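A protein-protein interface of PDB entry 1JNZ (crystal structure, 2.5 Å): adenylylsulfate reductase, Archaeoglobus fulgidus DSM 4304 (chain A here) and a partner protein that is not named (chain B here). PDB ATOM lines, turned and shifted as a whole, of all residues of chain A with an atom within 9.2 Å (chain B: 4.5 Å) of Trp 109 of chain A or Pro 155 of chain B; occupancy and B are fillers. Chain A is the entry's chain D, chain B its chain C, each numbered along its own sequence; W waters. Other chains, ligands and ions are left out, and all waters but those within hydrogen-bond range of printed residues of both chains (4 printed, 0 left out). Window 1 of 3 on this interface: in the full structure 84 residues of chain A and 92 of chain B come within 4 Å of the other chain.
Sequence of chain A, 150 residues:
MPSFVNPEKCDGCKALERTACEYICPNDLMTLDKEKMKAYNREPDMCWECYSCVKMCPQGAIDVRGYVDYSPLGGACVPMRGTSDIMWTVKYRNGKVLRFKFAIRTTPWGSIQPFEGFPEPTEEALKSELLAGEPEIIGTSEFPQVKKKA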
ATOM      1  N   TYR A  23     -20.257  16.403  41.634  1.00  0.00           N
ATOM      2  CA  TYR A  23     -18.807  16.309  41.670  1.00  0.00           C
ATOM      3  C   TYR A  23     -18.100  16.994  40.506  1.00  0.00           C
ATOM      4  O   TYR A  23     -17.104  17.692  40.699  1.00  0.00           O
ATOM      5  CB  TYR A  23     -18.395  14.832  41.691  1.00  0.00           C
ATOM      6  CG  TYR A  23     -16.994  14.578  41.171  1.00  0.00           C
ATOM      7  CD1 TYR A  23     -15.876  14.853  41.957  1.00  0.00           C
ATOM      8  CD2 TYR A  23     -16.789  14.106  39.874  1.00  0.00           C
ATOM      9  CE1 TYR A  23     -14.585  14.668  41.464  1.00  0.00           C
ATOM     10  CE2 TYR A  23     -15.505  13.920  39.371  1.00  0.00           C
ATOM     11  CZ  TYR A  23     -14.408  14.204  40.167  1.00  0.00           C
ATOM     12  OH  TYR A  23     -13.133  14.051  39.665  1.00  0.00           O
ATOM     13  N   ILE A  24     -18.633  16.791  39.305  1.00  0.00           N
ATOM     14  CA  ILE A  24     -18.035  17.306  38.082  1.00  0.00           C
ATOM     15  C   ILE A  24     -18.266  18.765  37.656  1.00  0.00           C
ATOM     16  O   ILE A  24     -17.374  19.373  37.068  1.00  0.00           O
ATOM     17  CB  ILE A  24     -18.428  16.378  36.895  1.00  0.00           C
ATOM     18  CG1 ILE A  24     -17.368  16.447  35.796  1.00  0.00           C
ATOM     19  CG2 ILE A  24     -19.790  16.771  36.347  1.00  0.00           C
ATOM     20  CD1 ILE A  24     -16.031  15.815  36.188  1.00  0.00           C
ATOM     21  N   SER A  52     -20.492  18.601  30.949  1.00  0.00           N
ATOM     22  CA  SER A  52     -19.687  17.721  31.800  1.00  0.00           C
ATOM     23  C   SER A  52     -20.598  16.795  32.604  1.00  0.00           C
ATOM     24  O   SER A  52     -20.358  15.591  32.699  1.00  0.00           O
ATOM     25  CB  SER A  52     -18.808  18.542  32.751  1.00  0.00           C
ATOM     26  OG  SER A  52     -17.757  19.177  32.048  1.00  0.00           O
ATOM     27  N   LYS A  55     -22.192  14.226  30.311  1.00  0.00           N
ATOM     28  CA  LYS A  55     -21.285  13.131  29.995  1.00  0.00           C
ATOM     29  C   LYS A  55     -20.986  12.200  31.169  1.00  0.00           C
ATOM     30  O   LYS A  55     -20.796  10.998  30.974  1.00  0.00           O
ATOM     31  CB  LYS A  55     -19.958  13.687  29.466  1.00  0.00           C
ATOM     32  CG  LYS A  55     -20.056  14.552  28.220  1.00  0.00           C
ATOM     33  CD  LYS A  55     -18.715  15.206  27.927  1.00  0.00           C
ATOM     34  CE  LYS A  55     -18.768  16.032  26.656  1.00  0.00           C
ATOM     35  NZ  LYS A  55     -17.518  16.811  26.459  1.00  0.00           N
ATOM     36  N   MET A  56     -20.960  12.722  32.391  1.00  0.00           N
ATOM     37  CA  MET A  56     -20.627  11.860  33.516  1.00  0.00           C
ATOM     38  C   MET A  56     -21.783  11.173  34.240  1.00  0.00           C
ATOM     39  O   MET A  56     -21.550  10.359  35.131  1.00  0.00           O
ATOM     40  CB  MET A  56     -19.765  12.633  34.517  1.00  0.00           C
ATOM     41  CG  MET A  56     -18.520  13.257  33.902  1.00  0.00           C
ATOM     42  SD  MET A  56     -17.679  12.176  32.703  1.00  0.00           S
ATOM     43  CE  MET A  56     -16.943  10.962  33.805  1.00  0.00           C
ATOM     44  N   ARG A  81     -20.285   9.000  25.874  1.00  0.00           N
ATOM     45  CA  ARG A  81     -18.846   8.958  26.083  1.00  0.00           C
ATOM     46  C   ARG A  81     -18.327   7.597  26.547  1.00  0.00           C
ATOM     47  O   ARG A  81     -18.817   7.027  27.522  1.00  0.00           O
ATOM     48  CB  ARG A  81     -18.457  10.049  27.087  1.00  0.00           C
ATOM     49  CG  ARG A  81     -16.972  10.288  27.227  1.00  0.00           C
ATOM     50  CD  ARG A  81     -16.705  11.614  27.917  1.00  0.00           C
ATOM     51  NE  ARG A  81     -15.291  11.787  28.225  1.00  0.00           N
ATOM     52  CZ  ARG A  81     -14.699  11.313  29.315  1.00  0.00           C
ATOM     53  NH1 ARG A  81     -15.402  10.638  30.215  1.00  0.00           N
ATOM     54  NH2 ARG A  81     -13.399  11.510  29.502  1.00  0.00           N
ATOM     55  N   GLY A  82     -17.331   7.085  25.835  1.00  0.00           N
ATOM     56  CA  GLY A  82     -16.750   5.803  26.185  1.00  0.00           C
ATOM     57  C   GLY A  82     -15.363   5.986  26.765  1.00  0.00           C
ATOM     58  O   GLY A  82     -15.093   6.974  27.449  1.00  0.00           O
ATOM     59  N   THR A  83     -14.467   5.045  26.489  1.00  0.00           N
ATOM     60  CA  THR A  83     -13.109   5.134  27.013  1.00  0.00           C
ATOM     61  C   THR A  83     -12.106   5.652  25.985  1.00  0.00           C
ATOM     62  O   THR A  83     -11.198   6.411  26.323  1.00  0.00           O
ATOM     63  CB  THR A  83     -12.633   3.769  27.525  1.00  0.00           C
ATOM     64  OG1 THR A  83     -12.794   2.800  26.488  1.00  0.00           O
ATOM     65  CG2 THR A  83     -13.436   3.338  28.751  1.00  0.00           C
ATOM     66  N   SER A  84     -12.271   5.244  24.731  1.00  0.00           N
ATOM     67  CA  SER A  84     -11.370   5.669  23.669  1.00  0.00           C
ATOM     68  C   SER A  84     -12.036   6.629  22.689  1.00  0.00           C
ATOM     69  O   SER A  84     -11.356   7.304  21.919  1.00  0.00           O
ATOM     70  CB  SER A  84     -10.843   4.453  22.903  1.00  0.00           C
ATOM     71  OG  SER A  84     -11.894   3.782  22.224  1.00  0.00           O
ATOM     72  N   ASP A  85     -13.365   6.685  22.709  1.00  0.00           N
ATOM     73  CA  ASP A  85     -14.085   7.574  21.808  1.00  0.00           C
ATOM     74  C   ASP A  85     -15.402   8.060  22.380  1.00  0.00           C
ATOM     75  O   ASP A  85     -15.845   7.606  23.436  1.00  0.00           O
ATOM     76  CB  ASP A  85     -14.327   6.892  20.455  1.00  0.00           C
ATOM     77  CG  ASP A  85     -14.980   5.527  20.590  1.00  0.00           C
ATOM     78  OD1 ASP A  85     -16.036   5.414  21.257  1.00  0.00           O
ATOM     79  OD2 ASP A  85     -14.439   4.555  20.014  1.00  0.00           O
ATOM     80  N   ILE A  86     -16.019   9.002  21.675  1.00  0.00           N
ATOM     81  CA  ILE A  86     -17.293   9.564  22.099  1.00  0.00           C
ATOM     82  C   ILE A  86     -18.244   9.628  20.912  1.00  0.00           C
ATOM     83  O   ILE A  86     -17.836   9.929  19.788  1.00  0.00           O
ATOM     84  CB  ILE A  86     -17.111  10.994  22.695  1.00  0.00           C
ATOM     85  CG1 ILE A  86     -18.443  11.509  23.243  1.00  0.00           C
ATOM     86  CG2 ILE A  86     -16.578  11.960  21.629  1.00  0.00           C
ATOM     87  CD1 ILE A  86     -18.331  12.844  23.958  1.00  0.00           C
ATOM     88  N   ALA A 103     -12.523  10.235  18.455  1.00  0.00           N
ATOM     89  CA  ALA A 103     -11.624   9.613  19.410  1.00  0.00           C
ATOM     90  C   ALA A 103     -11.421  10.634  20.527  1.00  0.00           C
ATOM     91  O   ALA A 103     -11.544  11.837  20.294  1.00  0.00           O
ATOM     92  CB  ALA A 103     -10.300   9.288  18.738  1.00  0.00           C
ATOM     93  N   ILE A 104     -11.123  10.163  21.736  1.00  0.00           N
ATOM     94  CA  ILE A 104     -10.914  11.066  22.867  1.00  0.00           C
ATOM     95  C   ILE A 104      -9.636  10.732  23.634  1.00  0.00           C
ATOM     96  O   ILE A 104      -9.159  11.531  24.444  1.00  0.00           O
ATOM     97  CB  ILE A 104     -12.099  11.010  23.858  1.00  0.00           C
ATOM     98  CG1 ILE A 104     -12.153   9.629  24.525  1.00  0.00           C
ATOM     99  CG2 ILE A 104     -13.403  11.315  23.129  1.00  0.00           C
ATOM    100  CD1 ILE A 104     -13.223   9.498  25.589  1.00  0.00           C
ATOM    101  N   ARG A 105      -9.094   9.545  23.389  1.00  0.00           N
ATOM    102  CA  ARG A 105      -7.866   9.130  24.052  1.00  0.00           C
ATOM    103  C   ARG A 105      -7.290   7.892  23.390  1.00  0.00           C
ATOM    104  O   ARG A 105      -8.019   6.963  23.046  1.00  0.00           O
ATOM    105  CB  ARG A 105      -8.109   8.863  25.542  1.00  0.00           C
ATOM    106  CG  ARG A 105      -6.823   8.589  26.308  1.00  0.00           C
ATOM    107  CD  ARG A 105      -6.992   8.779  27.800  1.00  0.00           C
ATOM    108  NE  ARG A 105      -5.723   8.582  28.494  1.00  0.00           N
ATOM    109  CZ  ARG A 105      -5.551   8.745  29.802  1.00  0.00           C
ATOM    110  NH1 ARG A 105      -6.569   9.106  30.569  1.00  0.00           N
ATOM    111  NH2 ARG A 105      -4.350   8.564  30.339  1.00  0.00           N
ATOM    112  N   THR A 106      -5.973   7.887  23.212  1.00  0.00           N
ATOM    113  CA  THR A 106      -5.294   6.772  22.567  1.00  0.00           C
ATOM    114  C   THR A 106      -4.625   5.826  23.558  1.00  0.00           C
ATOM    115  O   THR A 106      -3.989   4.858  23.154  1.00  0.00           O
ATOM    116  CB  THR A 106      -4.235   7.281  21.586  1.00  0.00           C
ATOM    117  OG1 THR A 106      -3.153   7.866  22.316  1.00  0.00           O
ATOM    118  CG2 THR A 106      -4.834   8.340  20.664  1.00  0.00           C
ATOM    119  N   THR A 107      -4.760   6.108  24.852  1.00  0.00           N
ATOM    120  CA  THR A 107      -4.179   5.260  25.886  1.00  0.00           C
ATOM    121  C   THR A 107      -5.225   4.908  26.946  1.00  0.00           C
ATOM    122  O   THR A 107      -6.264   5.566  27.055  1.00  0.00           O
ATOM    123  CB  THR A 107      -3.010   5.951  26.604  1.00  0.00           C
ATOM    124  OG1 THR A 107      -3.492   7.125  27.274  1.00  0.00           O
ATOM    125  CG2 THR A 107      -1.913   6.326  25.614  1.00  0.00           C
ATOM    126  N   PRO A 108      -4.963   3.863  27.743  1.00  0.00           N
ATOM    127  CA  PRO A 108      -5.919   3.466  28.785  1.00  0.00           C
ATOM    128  C   PRO A 108      -6.032   4.552  29.848  1.00  0.00           C
ATOM    129  O   PRO A 108      -5.057   5.249  30.129  1.00  0.00           O
ATOM    130  CB  PRO A 108      -5.310   2.179  29.347  1.00  0.00           C
ATOM    131  CG  PRO A 108      -4.561   1.615  28.155  1.00  0.00           C
ATOM    132  CD  PRO A 108      -3.900   2.854  27.589  1.00  0.00           C
ATOM    133  N   TRP A 109      -7.212   4.706  30.437  1.00  0.00           N
ATOM    134  CA  TRP A 109      -7.385   5.716  31.469  1.00  0.00           C
ATOM    135  C   TRP A 109      -6.615   5.363  32.737  1.00  0.00           C
ATOM    136  O   TRP A 109      -6.615   4.213  33.177  1.00  0.00           O
ATOM    137  CB  TRP A 109      -8.869   5.921  31.788  1.00  0.00           C
ATOM    138  CG  TRP A 109      -9.552   6.726  30.741  1.00  0.00           C
ATOM    139  CD1 TRP A 109     -10.090   6.265  29.570  1.00  0.00           C
ATOM    140  CD2 TRP A 109      -9.667   8.154  30.698  1.00  0.00           C
ATOM    141  NE1 TRP A 109     -10.522   7.315  28.798  1.00  0.00           N
ATOM    142  CE2 TRP A 109     -10.272   8.487  29.464  1.00  0.00           C
ATOM    143  CE3 TRP A 109      -9.308   9.185  31.577  1.00  0.00           C
ATOM    144  CZ2 TRP A 109     -10.532   9.811  29.089  1.00  0.00           C
ATOM    145  CZ3 TRP A 109      -9.565  10.508  31.202  1.00  0.00           C
ATOM    146  CH2 TRP A 109     -10.169  10.804  29.966  1.00  0.00           C
ATOM    147  N   GLY A 110      -5.951   6.366  33.306  1.00  0.00           N
ATOM    148  CA  GLY A 110      -5.176   6.172  34.520  1.00  0.00           C
ATOM    149  C   GLY A 110      -3.823   5.528  34.286  1.00  0.00           C
ATOM    150  O   GLY A 110      -3.177   5.079  35.228  1.00  0.00           O
ATOM    151  N   SER A 111      -3.377   5.499  33.033  1.00  0.00           N
ATOM    152  CA  SER A 111      -2.106   4.869  32.689  1.00  0.00           C
ATOM    153  C   SER A 111      -0.910   5.814  32.578  1.00  0.00           C
ATOM    154  O   SER A 111       0.198   5.375  32.269  1.00  0.00           O
ATOM    155  CB  SER A 111      -2.257   4.109  31.372  1.00  0.00           C
ATOM    156  OG  SER A 111      -2.631   4.991  30.332  1.00  0.00           O
ATOM    157  N   ILE A 112      -1.117   7.101  32.830  1.00  0.00           N
ATOM    158  CA  ILE A 112      -0.027   8.057  32.724  1.00  0.00           C
ATOM    159  C   ILE A 112       1.053   7.936  33.798  1.00  0.00           C
ATOM    160  O   ILE A 112       0.773   7.937  34.997  1.00  0.00           O
ATOM    161  CB  ILE A 112      -0.541   9.520  32.751  1.00  0.00           C
ATOM    162  CG1 ILE A 112      -1.426   9.803  31.539  1.00  0.00           C
ATOM    163  CG2 ILE A 112       0.651  10.487  32.793  1.00  0.00           C
ATOM    164  CD1 ILE A 112      -2.096  11.168  31.594  1.00  0.00           C
ATOM    165  N   GLU B  61     -10.792  17.540  37.249  1.00  0.00           N
ATOM    166  CA  GLU B  61     -11.125  16.720  36.088  1.00  0.00           C
ATOM    167  C   GLU B  61     -11.701  17.526  34.923  1.00  0.00           C
ATOM    168  O   GLU B  61     -11.394  17.249  33.766  1.00  0.00           O
ATOM    169  CB  GLU B  61     -12.113  15.610  36.470  1.00  0.00           C
ATOM    170  CG  GLU B  61     -12.166  14.478  35.445  1.00  0.00           C
ATOM    171  CD  GLU B  61     -13.143  13.381  35.818  1.00  0.00           C
ATOM    172  OE1 GLU B  61     -13.221  13.030  37.016  1.00  0.00           O
ATOM    173  OE2 GLU B  61     -13.820  12.855  34.909  1.00  0.00           O
ATOM    174  N   ARG B  62     -12.525  18.526  35.222  1.00  0.00           N
ATOM    175  CA  ARG B  62     -13.136  19.334  34.168  1.00  0.00           C
ATOM    176  C   ARG B  62     -13.123  20.843  34.423  1.00  0.00           C
ATOM    177  O   ARG B  62     -13.696  21.602  33.645  1.00  0.00           O
ATOM    178  CB  ARG B  62     -14.590  18.888  33.959  1.00  0.00           C
ATOM    179  CG  ARG B  62     -14.769  17.511  33.320  1.00  0.00           C
ATOM    180  CD  ARG B  62     -14.531  17.555  31.818  1.00  0.00           C
ATOM    181  NE  ARG B  62     -14.680  16.243  31.198  1.00  0.00           N
ATOM    182  CZ  ARG B  62     -14.686  16.026  29.884  1.00  0.00           C
ATOM    183  NH1 ARG B  62     -14.554  17.037  29.033  1.00  0.00           N
ATOM    184  NH2 ARG B  62     -14.821  14.789  29.420  1.00  0.00           N
ATOM    185  N   SER B 152     -11.543  15.089  25.773  1.00  0.00           N
ATOM    186  CA  SER B 152     -11.037  14.766  27.111  1.00  0.00           C
ATOM    187  C   SER B 152      -9.700  15.434  27.423  1.00  0.00           C
ATOM    188  O   SER B 152      -8.949  14.964  28.275  1.00  0.00           O
ATOM    189  CB  SER B 152     -10.885  13.249  27.275  1.00  0.00           C
ATOM    190  OG  SER B 152     -12.145  12.609  27.361  1.00  0.00           O
ATOM    191  N   TYR B 153      -9.427  16.542  26.744  1.00  0.00           N
ATOM    192  CA  TYR B 153      -8.188  17.293  26.913  1.00  0.00           C
ATOM    193  C   TYR B 153      -7.868  17.623  28.380  1.00  0.00           C
ATOM    194  O   TYR B 153      -6.742  17.415  28.829  1.00  0.00           O
ATOM    195  CB  TYR B 153      -8.269  18.566  26.057  1.00  0.00           C
ATOM    196  CG  TYR B 153      -6.961  19.297  25.805  1.00  0.00           C
ATOM    197  CD1 TYR B 153      -5.723  18.735  26.145  1.00  0.00           C
ATOM    198  CD2 TYR B 153      -6.967  20.554  25.197  1.00  0.00           C
ATOM    199  CE1 TYR B 153      -4.529  19.415  25.884  1.00  0.00           C
ATOM    200  CE2 TYR B 153      -5.793  21.235  24.933  1.00  0.00           C
ATOM    201  CZ  TYR B 153      -4.576  20.666  25.278  1.00  0.00           C
ATOM    202  OH  TYR B 153      -3.425  21.375  25.020  1.00  0.00           O
ATOM    203  N   LYS B 154      -8.853  18.120  29.127  1.00  0.00           N
ATOM    204  CA  LYS B 154      -8.670  18.457  30.535  1.00  0.00           C
ATOM    205  C   LYS B 154      -8.536  17.214  31.427  1.00  0.00           C
ATOM    206  O   LYS B 154      -7.660  17.167  32.284  1.00  0.00           O
ATOM    207  CB  LYS B 154      -9.807  19.356  31.042  1.00  0.00           C
ATOM    208  CG  LYS B 154      -9.576  19.876  32.471  1.00  0.00           C
ATOM    209  CD  LYS B 154      -8.298  20.732  32.567  1.00  0.00           C
ATOM    210  CE  LYS B 154      -7.778  20.851  34.004  1.00  0.00           C
ATOM    211  NZ  LYS B 154      -8.767  21.422  34.971  1.00  0.00           N
ATOM    212  N   PRO B 155      -9.435  16.229  31.272  1.00  0.00           N
ATOM    213  CA  PRO B 155      -9.342  15.021  32.099  1.00  0.00           C
ATOM    214  C   PRO B 155      -7.963  14.371  31.970  1.00  0.00           C
ATOM    215  O   PRO B 155      -7.435  13.813  32.933  1.00  0.00           O
ATOM    216  CB  PRO B 155     -10.455  14.137  31.542  1.00  0.00           C
ATOM    217  CG  PRO B 155     -11.469  15.128  31.093  1.00  0.00           C
ATOM    218  CD  PRO B 155     -10.644  16.202  30.429  1.00  0.00           C
ATOM    219  N   ILE B 156      -7.390  14.436  30.770  1.00  0.00           N
ATOM    220  CA  ILE B 156      -6.070  13.867  30.522  1.00  0.00           C
ATOM    221  C   ILE B 156      -5.002  14.661  31.273  1.00  0.00           C
ATOM    222  O   ILE B 156      -4.173  14.092  31.979  1.00  0.00           O
ATOM    223  CB  ILE B 156      -5.728  13.869  29.011  1.00  0.00           C
ATOM    224  CG1 ILE B 156      -6.688  12.946  28.264  1.00  0.00           C
ATOM    225  CG2 ILE B 156      -4.288  13.407  28.794  1.00  0.00           C
ATOM    226  CD1 ILE B 156      -6.400  12.820  26.783  1.00  0.00           C
ATOM    227  N   ILE B 157      -5.024  15.978  31.118  1.00  0.00           N
ATOM    228  CA  ILE B 157      -4.061  16.837  31.795  1.00  0.00           C
ATOM    229  C   ILE B 157      -4.277  16.773  33.307  1.00  0.00           C
ATOM    230  O   ILE B 157      -3.339  16.944  34.088  1.00  0.00           O
ATOM    231  CB  ILE B 157      -4.176  18.308  31.270  1.00  0.00           C
ATOM    232  CG1 ILE B 157      -3.120  18.546  30.186  1.00  0.00           C
ATOM    233  CG2 ILE B 157      -4.026  19.312  32.412  1.00  0.00           C
ATOM    234  CD1 ILE B 157      -3.154  17.534  29.061  1.00  0.00           C
ATOM    235  N   ALA B 158      -5.515  16.513  33.716  1.00  0.00           N
ATOM    236  CA  ALA B 158      -5.842  16.418  35.132  1.00  0.00           C
ATOM    237  C   ALA B 158      -5.208  15.151  35.710  1.00  0.00           C
ATOM    238  O   ALA B 158      -4.664  15.159  36.820  1.00  0.00           O
ATOM    239  CB  ALA B 158      -7.356  16.387  35.319  1.00  0.00           C
ATOM    240  N   GLU B 159      -5.275  14.067  34.944  1.00  0.00           N
ATOM    241  CA  GLU B 159      -4.705  12.795  35.370  1.00  0.00           C
ATOM    242  C   GLU B 159      -3.189  12.905  35.552  1.00  0.00           C
ATOM    243  O   GLU B 159      -2.628  12.379  36.515  1.00  0.00           O
ATOM    244  CB  GLU B 159      -5.032  11.705  34.343  1.00  0.00           C
ATOM    245  CG  GLU B 159      -4.435  10.348  34.675  1.00  0.00           C
ATOM    246  CD  GLU B 159      -4.795   9.284  33.664  1.00  0.00           C
ATOM    247  OE1 GLU B 159      -3.887   8.528  33.253  1.00  0.00           O
ATOM    248  OE2 GLU B 159      -5.984   9.197  33.288  1.00  0.00           O
HETATM  249  O   HOH W   1      -9.444  14.179  24.076  1.00  0.00           O
HETATM  250  O   HOH W   2     -14.706  13.614  32.500  1.00  0.00           O
HETATM  251  O   HOH W   3     -17.629  18.363  28.786  1.00  0.00           O
HETATM  252  O   HOH W   4     -11.162  16.036  39.690  1.00  0.00           O
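The side-chain carboxylate (OE1) of Glu 61 of chain B is in hydrogen-bond range of the side-chain hydroxyl (OH) of Tyr 23 of chain A (2.8 Å). NH2 of Arg 81 of chain A sits at hydrogen-bond distance from OG of Ser 152 of chain B (2.7 Å). The guanidinium group (NH1) of Arg 105 of chain A lies within salt-bridge range of the side-chain carboxylate (OE2) of Glu 159 of chain B. OE2 of Glu 159 of chain B is in hydrogen-bond range of N of Gly 110 of chain A. The side-chain carboxylate (OE1) of Glu 159 of chain B is in hydrogen-bond range of the backbone NH (N) of Ser 111 of chain A (3.1 Å). OE1 of Glu 159 of chain B lies within hydrogen-bond range of N of Ile 112 of chain A. The guanidinium group (NE) of Arg 81 of chain A lies close to the guanidinium group (NH2) of Arg 62 of chain B.
The guanidinium group (NH1) of Arg 81 of chain A sits at hydrogen-bond distance from the side-chain sulfur (SD) of Met 56 of chain A, 3.7 Å away. The indole nitrogen of Trp 109 of chain A sits at hydrogen-bond distance from the backbone carbonyl oxygen of Thr 83 of chain A (2.7 Å). O of Ser 84 of chain A is in hydrogen-bond range of N of Ile 104 of chain A, 2.9 Å away. The side-chain hydroxyl (OG1) of Thr 107 of chain A lies within hydrogen-bond range of the guanidinium group (NE) of Arg 105 of chain A (2.9 Å). NH2 of Arg 105 of chain A lies within hydrogen-bond range of O of Pro 108 of chain A (3.4 Å). The side-chain hydroxyl (OG) of Ser 111 of chain A is in hydrogen-bond range of the backbone carbonyl oxygen (O) of Pro 108 of chain A, at 2.4 Å.
CD1 of Ile 24 of chain A touches CD of Glu 61 of chain B, 3.8 Å away. Arg 62 of chain B touches Ile 24 of chain A. CD of Arg 62 of chain B touches OG of Ser 52 of chain A (3.6 Å). Lys 55 of chain A touches Arg 62 of chain B. Glu 61 of chain B touches Met 56 of chain A. Ile 104 of chain A touches Ile 156 of chain B. Trp 109 of chain A touches Ser 152 of chain B (CZ2 to OG, 3.7 Å). Trp 109 of chain A touches Pro 155 of chain B (CH2 to CB, 3.7 Å). Trp 109 of chain A touches Glu 159 of chain B. CD1 of Ile 112 of chain A touches O of Ile 156 of chain B, 3.6 Å away.
Of chain B, only Ser 152, Pro 155 and Glu 159 come within 4 Å of Trp 109 of chain A. Pro 155 of chain B touches just one residue of chain A: Trp 109. No residue of chain A comes within 4 Å of Ala 158 of chain B. Of the printed residues of chain B, Ile 112 of chain A touches Ile 156 and Glu 159. Printed residues of chain B within 4 Å of Ile 24 of chain A: Glu 61 (3.8 Å) and Arg 62 (3.6 Å). Ser 84 of chain A touches none of the printed residues of chain B. The nearest residue of chain A that does not touch Pro 155 of chain B is Arg 81 of chain A (4.4 Å). The nearest printed residue of chain B that does not touch Lys 55 of chain A is Ser 152 of chain B (6.3 Å).
Printed residues of chain A that touch a printed residue of chain B: Tyr 23, Ile 24, Ser 52, Lys 55, Met 56, Arg 81, Ile 104, Arg 105, Trp 109, Gly 110, Ser 111 and Ile 112. Hydrophobic or aromatic side chains of chain A that line the printed part of chain B: Tyr 23, Ile 24, Met 56, Ile 104, Trp 109 and Ile 112. Printed residues of chain B that touch a printed residue of chain A: Glu 61, Arg 62, Ser 152, Pro 155, Ile 156 and Glu 159. Hydrophobic or aromatic side chains of chain B within 4 Å of the printed part of chain A: Pro 155 and Ile 156.
Water W2 lies within hydrogen-bond range of OE2 of Glu 61 of chain B (2.7 Å), NE of Arg 62 of chain B (2.9 Å) and SD of Met 56 of chain A (3.3 Å). Water W1 lies within hydrogen-bond range of the backbone carbonyl oxygen of Ile 104 of chain A and the backbone NH of Ser 152 of chain B. Water W4 lies within hydrogen-bond range of OH of Tyr 23 of chain A (2.8 Å) and N of Glu 61 of chain B (2.9 Å). Water W3 lies within hydrogen-bond range of the side-chain amino group (NZ) of Lys 55 of chain A (2.8 Å), the guanidinium group (NH1) of Arg 62 of chain B (3.4 Å) and the side-chain hydroxyl (OG) of Ser 52 of chain A (3.4 Å).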
